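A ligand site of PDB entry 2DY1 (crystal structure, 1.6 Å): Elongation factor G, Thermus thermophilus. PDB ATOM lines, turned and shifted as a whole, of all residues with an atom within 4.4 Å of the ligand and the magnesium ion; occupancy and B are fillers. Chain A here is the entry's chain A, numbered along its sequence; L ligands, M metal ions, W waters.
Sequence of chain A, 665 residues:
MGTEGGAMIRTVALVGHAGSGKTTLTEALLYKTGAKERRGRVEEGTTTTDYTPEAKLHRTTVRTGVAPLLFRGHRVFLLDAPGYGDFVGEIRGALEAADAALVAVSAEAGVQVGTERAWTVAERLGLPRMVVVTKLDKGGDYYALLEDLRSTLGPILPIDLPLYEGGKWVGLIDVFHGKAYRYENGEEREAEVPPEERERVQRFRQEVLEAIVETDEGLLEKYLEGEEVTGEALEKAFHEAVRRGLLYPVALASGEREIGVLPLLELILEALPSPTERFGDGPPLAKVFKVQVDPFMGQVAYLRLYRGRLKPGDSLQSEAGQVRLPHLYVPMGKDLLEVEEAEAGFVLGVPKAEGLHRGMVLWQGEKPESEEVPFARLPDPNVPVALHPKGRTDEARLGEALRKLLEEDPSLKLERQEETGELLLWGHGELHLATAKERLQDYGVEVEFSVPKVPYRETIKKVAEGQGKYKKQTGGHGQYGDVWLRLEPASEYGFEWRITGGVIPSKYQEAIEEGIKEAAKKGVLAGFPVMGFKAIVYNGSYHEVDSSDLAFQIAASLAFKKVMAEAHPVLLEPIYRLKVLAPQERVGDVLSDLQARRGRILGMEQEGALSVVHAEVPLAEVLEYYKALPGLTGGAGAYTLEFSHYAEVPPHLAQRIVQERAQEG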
ATOM      1  N   HIS A  17      20.483 -11.236  10.916  1.00  0.00           N
ATOM      2  CA  HIS A  17      20.503 -12.541  11.551  1.00  0.00           C
ATOM      3  C   HIS A  17      19.146 -12.922  12.096  1.00  0.00           C
ATOM      4  O   HIS A  17      18.341 -12.071  12.487  1.00  0.00           O
ATOM      5  CB  HIS A  17      21.499 -12.532  12.705  1.00  0.00           C
ATOM      6  CG  HIS A  17      21.903 -13.903  13.177  1.00  0.00           C
ATOM      7  ND1 HIS A  17      22.917 -14.622  12.595  1.00  0.00           N
ATOM      8  CD2 HIS A  17      21.428 -14.667  14.184  1.00  0.00           C
ATOM      9  CE1 HIS A  17      23.046 -15.780  13.213  1.00  0.00           C
ATOM     10  NE2 HIS A  17      22.157 -15.829  14.187  1.00  0.00           N
ATOM     11  N   ALA A  18      18.919 -14.229  12.162  1.00  0.00           N
ATOM     12  CA  ALA A  18      17.669 -14.742  12.689  1.00  0.00           C
ATOM     13  C   ALA A  18      17.378 -14.153  14.069  1.00  0.00           C
ATOM     14  O   ALA A  18      18.250 -14.130  14.946  1.00  0.00           O
ATOM     15  CB  ALA A  18      17.763 -16.259  12.769  1.00  0.00           C
ATOM     16  N   GLY A  19      16.151 -13.683  14.263  1.00  0.00           N
ATOM     17  CA  GLY A  19      15.720 -13.147  15.541  1.00  0.00           C
ATOM     18  C   GLY A  19      16.161 -11.730  15.868  1.00  0.00           C
ATOM     19  O   GLY A  19      15.999 -11.296  17.011  1.00  0.00           O
ATOM     20  N   SER A  20      16.701 -11.019  14.888  1.00  0.00           N
ATOM     21  CA  SER A  20      17.163  -9.649  15.102  1.00  0.00           C
ATOM     22  C   SER A  20      16.020  -8.617  15.163  1.00  0.00           C
ATOM     23  O   SER A  20      16.282  -7.428  15.295  1.00  0.00           O
ATOM     24  CB  SER A  20      18.187  -9.270  14.021  1.00  0.00           C
ATOM     25  OG  SER A  20      17.670  -9.437  12.721  1.00  0.00           O
ATOM     26  N   GLY A  21      14.772  -9.056  15.042  1.00  0.00           N
ATOM     27  CA  GLY A  21      13.639  -8.157  15.174  1.00  0.00           C
ATOM     28  C   GLY A  21      13.015  -7.582  13.925  1.00  0.00           C
ATOM     29  O   GLY A  21      12.255  -6.632  14.003  1.00  0.00           O
ATOM     30  N   LYS A  22      13.330  -8.191  12.780  1.00  0.00           N
ATOM     31  CA  LYS A  22      12.842  -7.729  11.483  1.00  0.00           C
ATOM     32  C   LYS A  22      11.321  -7.738  11.328  1.00  0.00           C
ATOM     33  O   LYS A  22      10.691  -6.726  10.986  1.00  0.00           O
ATOM     34  CB  LYS A  22      13.467  -8.587  10.370  1.00  0.00           C
ATOM     35  CG  LYS A  22      15.021  -8.491  10.304  1.00  0.00           C
ATOM     36  CD  LYS A  22      15.605  -9.399   9.203  1.00  0.00           C
ATOM     37  CE  LYS A  22      15.303 -10.888   9.392  1.00  0.00           C
ATOM     38  NZ  LYS A  22      16.052 -11.521  10.506  1.00  0.00           N
ATOM     39  N   THR A  23      10.708  -8.891  11.588  1.00  0.00           N
ATOM     40  CA  THR A  23       9.274  -8.963  11.419  1.00  0.00           C
ATOM     41  C   THR A  23       8.541  -8.117  12.423  1.00  0.00           C
ATOM     42  O   THR A  23       7.509  -7.536  12.132  1.00  0.00           O
ATOM     43  CB  THR A  23       8.845 -10.435  11.490  1.00  0.00           C
ATOM     44  OG1 THR A  23       9.477 -11.124  10.406  1.00  0.00           O
ATOM     45  CG2 THR A  23       7.303 -10.585  11.377  1.00  0.00           C
ATOM     46  N   THR A  24       9.096  -8.017  13.635  1.00  0.00           N
ATOM     47  CA  THR A  24       8.470  -7.196  14.674  1.00  0.00           C
ATOM     48  C   THR A  24       8.525  -5.701  14.276  1.00  0.00           C
ATOM     49  O   THR A  24       7.588  -4.942  14.522  1.00  0.00           O
ATOM     50  CB  THR A  24       9.175  -7.475  16.005  1.00  0.00           C
ATOM     51  OG1 THR A  24       8.990  -8.854  16.352  1.00  0.00           O
ATOM     52  CG2 THR A  24       8.587  -6.608  17.119  1.00  0.00           C
ATOM     53  N   VAL A  42       4.849 -12.094  16.581  1.00  0.00           N
ATOM     54  CA  VAL A  42       5.417 -13.344  16.073  1.00  0.00           C
ATOM     55  C   VAL A  42       5.044 -14.508  17.001  1.00  0.00           C
ATOM     56  O   VAL A  42       4.655 -15.581  16.551  1.00  0.00           O
ATOM     57  CB  VAL A  42       6.952 -13.255  15.959  1.00  0.00           C
ATOM     58  CG1 VAL A  42       7.552 -14.626  15.735  1.00  0.00           C
ATOM     59  CG2 VAL A  42       7.323 -12.323  14.813  1.00  0.00           C
ATOM     60  N   GLU A  43       5.151 -14.269  18.314  1.00  0.00           N
ATOM     61  CA  GLU A  43       4.837 -15.306  19.295  1.00  0.00           C
ATOM     62  C   GLU A  43       3.368 -15.734  19.310  1.00  0.00           C
ATOM     63  O   GLU A  43       3.021 -16.757  19.917  1.00  0.00           O
ATOM     64  CB  GLU A  43       5.259 -14.819  20.701  1.00  0.00           C
ATOM     65  CG  GLU A  43       4.419 -13.651  21.181  1.00  0.00           C
ATOM     66  CD  GLU A  43       5.042 -12.269  20.951  1.00  0.00           C
ATOM     67  OE1 GLU A  43       5.784 -12.075  19.952  1.00  0.00           O
ATOM     68  OE2 GLU A  43       4.758 -11.370  21.780  1.00  0.00           O
ATOM     69  N   ASP A  50       4.746 -13.419   8.495  1.00  0.00           N
ATOM     70  CA  ASP A  50       4.752 -14.821   8.785  1.00  0.00           C
ATOM     71  C   ASP A  50       3.339 -15.410   8.779  1.00  0.00           C
ATOM     72  O   ASP A  50       2.657 -15.457   9.795  1.00  0.00           O
ATOM     73  CB  ASP A  50       5.463 -15.051  10.127  1.00  0.00           C
ATOM     74  CG  ASP A  50       6.967 -14.683  10.073  1.00  0.00           C
ATOM     75  OD1 ASP A  50       7.535 -14.508   8.959  1.00  0.00           O
ATOM     76  OD2 ASP A  50       7.620 -14.621  11.145  1.00  0.00           O
ATOM     77  N   ARG A  59       8.352 -20.290  13.948  1.00  0.00           N
ATOM     78  CA  ARG A  59       8.497 -18.932  14.480  1.00  0.00           C
ATOM     79  C   ARG A  59       9.695 -18.214  13.856  1.00  0.00           C
ATOM     80  O   ARG A  59      10.509 -17.603  14.551  1.00  0.00           O
ATOM     81  CB  ARG A  59       8.620 -18.982  16.019  1.00  0.00           C
ATOM     82  CG  ARG A  59       7.354 -19.482  16.737  1.00  0.00           C
ATOM     83  CD  ARG A  59       6.215 -18.472  16.589  1.00  0.00           C
ATOM     84  NE  ARG A  59       5.086 -18.652  17.511  1.00  0.00           N
ATOM     85  CZ  ARG A  59       3.837 -18.952  17.135  1.00  0.00           C
ATOM     86  NH1 ARG A  59       3.524 -19.127  15.854  1.00  0.00           N
ATOM     87  NH2 ARG A  59       2.873 -18.977  18.051  1.00  0.00           N
ATOM     88  N   THR A  60       9.785 -18.289  12.529  1.00  0.00           N
ATOM     89  CA  THR A  60      10.864 -17.643  11.799  1.00  0.00           C
ATOM     90  C   THR A  60      10.338 -17.317  10.412  1.00  0.00           C
ATOM     91  O   THR A  60       9.450 -17.993   9.895  1.00  0.00           O
ATOM     92  CB  THR A  60      12.116 -18.558  11.721  1.00  0.00           C
ATOM     93  OG1 THR A  60      13.228 -17.820  11.166  1.00  0.00           O
ATOM     94  CG2 THR A  60      11.848 -19.759  10.822  1.00  0.00           C
ATOM     95  N   THR A  61      10.877 -16.279   9.787  1.00  0.00           N
ATOM     96  CA  THR A  61      10.435 -15.927   8.453  1.00  0.00           C
ATOM     97  C   THR A  61      11.037 -16.888   7.434  1.00  0.00           C
ATOM     98  O   THR A  61      12.213 -16.810   7.088  1.00  0.00           O
ATOM     99  CB  THR A  61      10.839 -14.457   8.182  1.00  0.00           C
ATOM    100  OG1 THR A  61      10.103 -13.638   9.091  1.00  0.00           O
ATOM    101  CG2 THR A  61      10.494 -14.034   6.740  1.00  0.00           C
ATOM    102  N   ASP A  80      10.375  -7.925   4.023  1.00  0.00           N
ATOM    103  CA  ASP A  80      10.773  -8.504   5.313  1.00  0.00           C
ATOM    104  C   ASP A  80      11.282  -9.909   5.004  1.00  0.00           C
ATOM    105  O   ASP A  80      10.505 -10.850   4.783  1.00  0.00           O
ATOM    106  CB  ASP A  80       9.538  -8.512   6.255  1.00  0.00           C
ATOM    107  CG  ASP A  80       9.816  -9.150   7.597  1.00  0.00           C
ATOM    108  OD1 ASP A  80      11.004  -9.238   7.956  1.00  0.00           O
ATOM    109  OD2 ASP A  80       8.846  -9.567   8.291  1.00  0.00           O
ATOM    110  N   PRO A  82      13.940 -13.482   5.308  1.00  0.00           N
ATOM    111  CA  PRO A  82      14.346 -14.482   6.305  1.00  0.00           C
ATOM    112  C   PRO A  82      15.667 -14.094   6.951  1.00  0.00           C
ATOM    113  O   PRO A  82      16.419 -13.236   6.450  1.00  0.00           O
ATOM    114  CB  PRO A  82      14.537 -15.749   5.482  1.00  0.00           C
ATOM    115  CG  PRO A  82      13.568 -15.578   4.332  1.00  0.00           C
ATOM    116  CD  PRO A  82      13.778 -14.110   3.986  1.00  0.00           C
ATOM    117  N   GLY A  83      15.971 -14.773   8.045  1.00  0.00           N
ATOM    118  CA  GLY A  83      17.213 -14.544   8.735  1.00  0.00           C
ATOM    119  C   GLY A  83      18.128 -15.767   8.586  1.00  0.00           C
ATOM    120  O   GLY A  83      19.331 -15.637   8.442  1.00  0.00           O
ATOM    121  N   THR A 134      18.162  -3.024  17.093  1.00  0.00           N
ATOM    122  CA  THR A 134      16.981  -3.466  17.830  1.00  0.00           C
ATOM    123  C   THR A 134      17.343  -4.047  19.191  1.00  0.00           C
ATOM    124  O   THR A 134      18.515  -4.213  19.509  1.00  0.00           O
ATOM    125  CB  THR A 134      16.290  -4.590  17.072  1.00  0.00           C
ATOM    126  OG1 THR A 134      17.232  -5.673  16.926  1.00  0.00           O
ATOM    127  CG2 THR A 134      15.828  -4.095  15.688  1.00  0.00           C
ATOM    128  N   LYS A 135      16.310  -4.356  19.970  1.00  0.00           N
ATOM    129  CA  LYS A 135      16.480  -4.999  21.276  1.00  0.00           C
ATOM    130  C   LYS A 135      17.362  -4.322  22.326  1.00  0.00           C
ATOM    131  O   LYS A 135      17.845  -4.981  23.255  1.00  0.00           O
ATOM    132  CB  LYS A 135      16.984  -6.437  21.052  1.00  0.00           C
ATOM    133  CG  LYS A 135      16.049  -7.289  20.196  1.00  0.00           C
ATOM    134  CD  LYS A 135      16.497  -8.763  20.176  1.00  0.00           C
ATOM    135  CE  LYS A 135      15.452  -9.670  19.534  1.00  0.00           C
ATOM    136  NZ  LYS A 135      15.764 -11.147  19.689  1.00  0.00           N
ATOM    137  N   ASP A 137      16.384  -2.654  24.597  1.00  0.00           N
ATOM    138  CA  ASP A 137      15.643  -2.729  25.867  1.00  0.00           C
ATOM    139  C   ASP A 137      16.076  -3.933  26.690  1.00  0.00           C
ATOM    140  O   ASP A 137      15.791  -4.008  27.886  1.00  0.00           O
ATOM    141  CB  ASP A 137      14.138  -2.776  25.628  1.00  0.00           C
ATOM    142  CG  ASP A 137      13.715  -3.943  24.749  1.00  0.00           C
ATOM    143  OD1 ASP A 137      14.243  -4.047  23.611  1.00  0.00           O
ATOM    144  OD2 ASP A 137      12.854  -4.745  25.194  1.00  0.00           O
ATOM    145  N   LYS A 138      16.748  -4.870  26.046  1.00  0.00           N
ATOM    146  CA  LYS A 138      17.210  -6.051  26.767  1.00  0.00           C
ATOM    147  C   LYS A 138      18.486  -5.778  27.581  1.00  0.00           C
ATOM    148  O   LYS A 138      18.940  -6.649  28.324  1.00  0.00           O
ATOM    149  CB  LYS A 138      17.362  -7.222  25.795  1.00  0.00           C
ATOM    150  CG  LYS A 138      16.029  -7.538  25.113  1.00  0.00           C
ATOM    151  CD  LYS A 138      16.060  -8.778  24.230  1.00  0.00           C
ATOM    152  CE  LYS A 138      15.930 -10.065  25.037  1.00  0.00           C
ATOM    153  NZ  LYS A 138      15.906 -11.263  24.144  1.00  0.00           N
ATOM    154  N   SER A 254      12.832  -0.091  17.833  1.00  0.00           N
ATOM    155  CA  SER A 254      12.358  -1.377  18.341  1.00  0.00           C
ATOM    156  C   SER A 254      10.857  -1.463  18.072  1.00  0.00           C
ATOM    157  O   SER A 254      10.092  -0.594  18.450  1.00  0.00           O
ATOM    158  CB  SER A 254      12.587  -1.509  19.841  1.00  0.00           C
ATOM    159  OG  SER A 254      11.817  -2.586  20.353  1.00  0.00           O
ATOM    160  N   GLU A 256       9.076  -3.818  19.294  1.00  0.00           N
ATOM    161  CA  GLU A 256       8.512  -4.397  20.527  1.00  0.00           C
ATOM    162  C   GLU A 256       8.233  -3.295  21.543  1.00  0.00           C
ATOM    163  O   GLU A 256       7.179  -3.276  22.161  1.00  0.00           O
ATOM    164  CB  GLU A 256       9.500  -5.408  21.099  1.00  0.00           C
ATOM    165  CG  GLU A 256       8.964  -6.284  22.213  1.00  0.00           C
ATOM    166  CD  GLU A 256       8.025  -7.349  21.695  1.00  0.00           C
ATOM    167  OE1 GLU A 256       8.338  -7.940  20.636  1.00  0.00           O
ATOM    168  OE2 GLU A 256       6.991  -7.602  22.345  1.00  0.00           O
HETATM  169  P1  LIG L   1      13.687 -14.187  11.665  1.00  0.00           P
HETATM  170  O1  LIG L   1      13.533 -15.666  12.275  1.00  0.00           O
HETATM  171  O2  LIG L   1      12.480 -13.914  10.644  1.00  0.00           O
HETATM  172  O3  LIG L   1      15.010 -13.953  11.051  1.00  0.00           O
HETATM  173  O4  LIG L   1      13.448 -13.256  12.959  1.00  0.00           O
HETATM  174  P2  LIG L   1      13.117 -11.693  12.918  1.00  0.00           P
HETATM  175  O5  LIG L   1      14.373 -10.950  12.653  1.00  0.00           O
HETATM  176  O6  LIG L   1      11.973 -11.446  12.010  1.00  0.00           O
HETATM  177  O7  LIG L   1      12.756 -11.398  14.449  1.00  0.00           O
HETATM  178  P3  LIG L   1      11.265 -11.406  15.044  1.00  0.00           P
HETATM  179  O8  LIG L   1      10.586 -10.151  14.664  1.00  0.00           O
HETATM  180  O9  LIG L   1      10.623 -12.696  14.702  1.00  0.00           O
HETATM  181  O10 LIG L   1      11.519 -11.341  16.634  1.00  0.00           O
HETATM  182  C1  LIG L   1      12.009 -12.521  17.288  1.00  0.00           C
HETATM  183  C2  LIG L   1      11.827 -12.370  18.800  1.00  0.00           C
HETATM  184  O11 LIG L   1      12.440 -11.130  19.171  1.00  0.00           O
HETATM  185  C3  LIG L   1      10.335 -12.239  19.139  1.00  0.00           C
HETATM  186  O12 LIG L   1      10.105 -12.790  20.440  1.00  0.00           O
HETATM  187  C4  LIG L   1      10.127 -10.732  19.158  1.00  0.00           C
HETATM  188  O13 LIG L   1       9.065 -10.413  20.050  1.00  0.00           O
HETATM  189  C5  LIG L   1      11.446 -10.314  19.818  1.00  0.00           C
HETATM  190  N1  LIG L   1      11.779  -8.894  19.604  1.00  0.00           N
HETATM  191  C6  LIG L   1      11.848  -8.263  18.439  1.00  0.00           C
HETATM  192  N2  LIG L   1      12.306  -7.032  18.612  1.00  0.00           N
HETATM  193  C7  LIG L   1      12.527  -6.855  19.918  1.00  0.00           C
HETATM  194  C8  LIG L   1      12.991  -5.796  20.679  1.00  0.00           C
HETATM  195  O14 LIG L   1      13.349  -4.736  20.163  1.00  0.00           O
HETATM  196  N3  LIG L   1      13.083  -5.959  22.063  1.00  0.00           N
HETATM  197  C9  LIG L   1      12.719  -7.171  22.646  1.00  0.00           C
HETATM  198  N4  LIG L   1      12.809  -7.332  23.973  1.00  0.00           N
HETATM  199  N5  LIG L   1      12.279  -8.181  21.884  1.00  0.00           N
HETATM  200  C10 LIG L   1      12.176  -8.040  20.554  1.00  0.00           C
HETATM  201 MG    MG M   1      11.064 -12.548  10.545  1.00  0.00          MG
HETATM  202  O   HOH W   1      12.065 -11.452   9.062  1.00  0.00           O
HETATM  203  O   HOH W   2       6.283  -9.447  19.707  1.00  0.00           O
HETATM  204  O   HOH W   3      11.860  -9.588  25.379  1.00  0.00           O
HETATM  205  O   HOH W   4      11.831  -4.882  16.584  1.00  0.00           O
HETATM  206  O   HOH W   5       9.060 -15.494  19.108  1.00  0.00           O
HETATM  207  O   HOH W   6      12.003 -12.847  22.408  1.00  0.00           O
HETATM  208  O   HOH W   7      14.034 -16.630  14.677  1.00  0.00           O
HETATM  209  O   HOH W   8      11.711 -15.306  14.841  1.00  0.00           O
HETATM  210  O   HOH W   9      13.917 -11.193  22.166  1.00  0.00           O
HETATM  211  O   HOH W  10      13.459 -15.467  17.036  1.00  0.00           O
HETATM  212  O   HOH W  11      14.780 -14.023  18.919  1.00  0.00           O
HETATM  213  O   HOH W  12       9.887 -13.487  11.996  1.00  0.00           O
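O2 of the ligand sits close to N of Thr 61 (3.0 Å).
O8 of the ligand sits at hydrogen-bond distance from N of Thr 23 (3.3 Å).
The side-chain hydroxyl (OG1) of Thr 60 is in hydrogen-bond range of an oxygen (O1) of the ligand, 2.4 Å away.
An oxygen (O13) of the ligand lies within hydrogen-bond range of the side-chain carboxylate (OE1) of Glu 256.
O14 of the ligand sits at hydrogen-bond distance from OG of Ser 254 (2.6 Å).
N of Thr 24 is in hydrogen-bond range of O8 of the ligand.
An oxygen (O8) of the ligand lies within hydrogen-bond range of the side-chain hydroxyl (OG1) of Thr 24, 2.7 Å away.
N of Lys 22 is in hydrogen-bond range of O5 of the ligand, at 3.0 Å.
An oxygen (O3) of the ligand is in salt-bridge range of the side-chain amino group of Lys 22.
N3 of the ligand is in hydrogen-bond range of OD1 of Asp 137 (2.7 Å).
N of Lys 135 lies within hydrogen-bond range of O14 of the ligand (3.0 Å).
An oxygen (O11) of the ligand lies within hydrogen-bond range of the side-chain amino group of Lys 135 (3.4 Å).
An oxygen (O4) of the ligand sits at hydrogen-bond distance from the backbone NH (N) of Gly 19 (3.0 Å).
The backbone NH (N) of Gly 21 lies within hydrogen-bond range of an oxygen (O5) of the ligand, 3.1 Å away.
O5 of the ligand is in hydrogen-bond range of N of Ser 20, at 3.2 Å.
The backbone NH (N) of Gly 83 sits close to an oxygen (O3) of the ligand (3.3 Å).
OD1 of Asp 50 sits close to OG1 of Thr 61, at 2.7 Å.
OG1 of Thr 23 lies close to OD2 of Asp 80 (2.7 Å).
The backbone NH (N) of Glu 256 is in hydrogen-bond range of the side-chain hydroxyl (OG) of Ser 254 (3.2 Å).
The side-chain amino group (NZ) of Lys 22 is in hydrogen-bond range of the side-chain hydroxyl (OG) of Ser 20.
The side-chain amino group of Lys 135 lies within hydrogen-bond range of the backbone carbonyl oxygen of Gly 19 (2.7 Å).
The side-chain hydroxyl of Thr 134 lies within hydrogen-bond range of the backbone carbonyl oxygen of Ser 20 (2.6 Å).
The backbone carbonyl oxygen (O) of Val 42 is in hydrogen-bond range of the guanidinium group (NE) of Arg 59, at 3.2 Å.
The backbone carbonyl oxygen (O) of Glu 43 is in hydrogen-bond range of the guanidinium group (NH2) of Arg 59 (2.9 Å).
Merely in contact with the ligand: Ala 18, Val 42, Glu 43 and Lys 138.
Hydrophobic or aromatic side chains within 4 Å of the ligand: Ala 18 and Val 42.
Within 4 Å of the ligand: Ala 18, Gly 19, Ser 20, Gly 21, Lys 22, Thr 23, Thr 24, Val 42, Glu 43, Thr 60, Thr 61, Gly 83, Lys 135, Asp 137, Lys 138, Ser 254 and Glu 256.
Within 4 Å of the magnesium ion: Thr 23 and Thr 61.
The nearest printed residue that does not touch the magnesium ion is Asp 50 (4.1 Å).
O2 of the ligand is bound to the magnesium ion, at 2.0 Å.
The magnesium ion is bound by O6 of the ligand (2.0 Å).
OG1 of Thr 61 is bound to the magnesium ion (2.1 Å).
Water W12 binds the magnesium ion (2.1 Å).
The magnesium ion is bound by water W1 (2.1 Å).
The side-chain hydroxyl (OG1) of Thr 23 binds the magnesium ion (2.1 Å).
Water W12 lies within hydrogen-bond range of OD2 of Asp 50 and O9 of the ligand.
Water W8 bridges the backbone carbonyl oxygen of Arg 59 and an oxygen (O9) of the ligand.
Water W2 lies within hydrogen-bond range of the side-chain carboxylate (OE1) of Glu 43 (2.7 Å), the side-chain carboxylate (OE1) of Glu 256 (2.7 Å) and an oxygen (O13) of the ligand (3.0 Å).
Water W4 lies within hydrogen-bond range of a nitrogen (N2) of the ligand and the backbone carbonyl oxygen of Gly 21.
Water W9 lies within hydrogen-bond range of NZ of Lys 138 (2.8 Å), NZ of Lys 135 (3.1 Å) and O11 of the ligand (3.3 Å).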
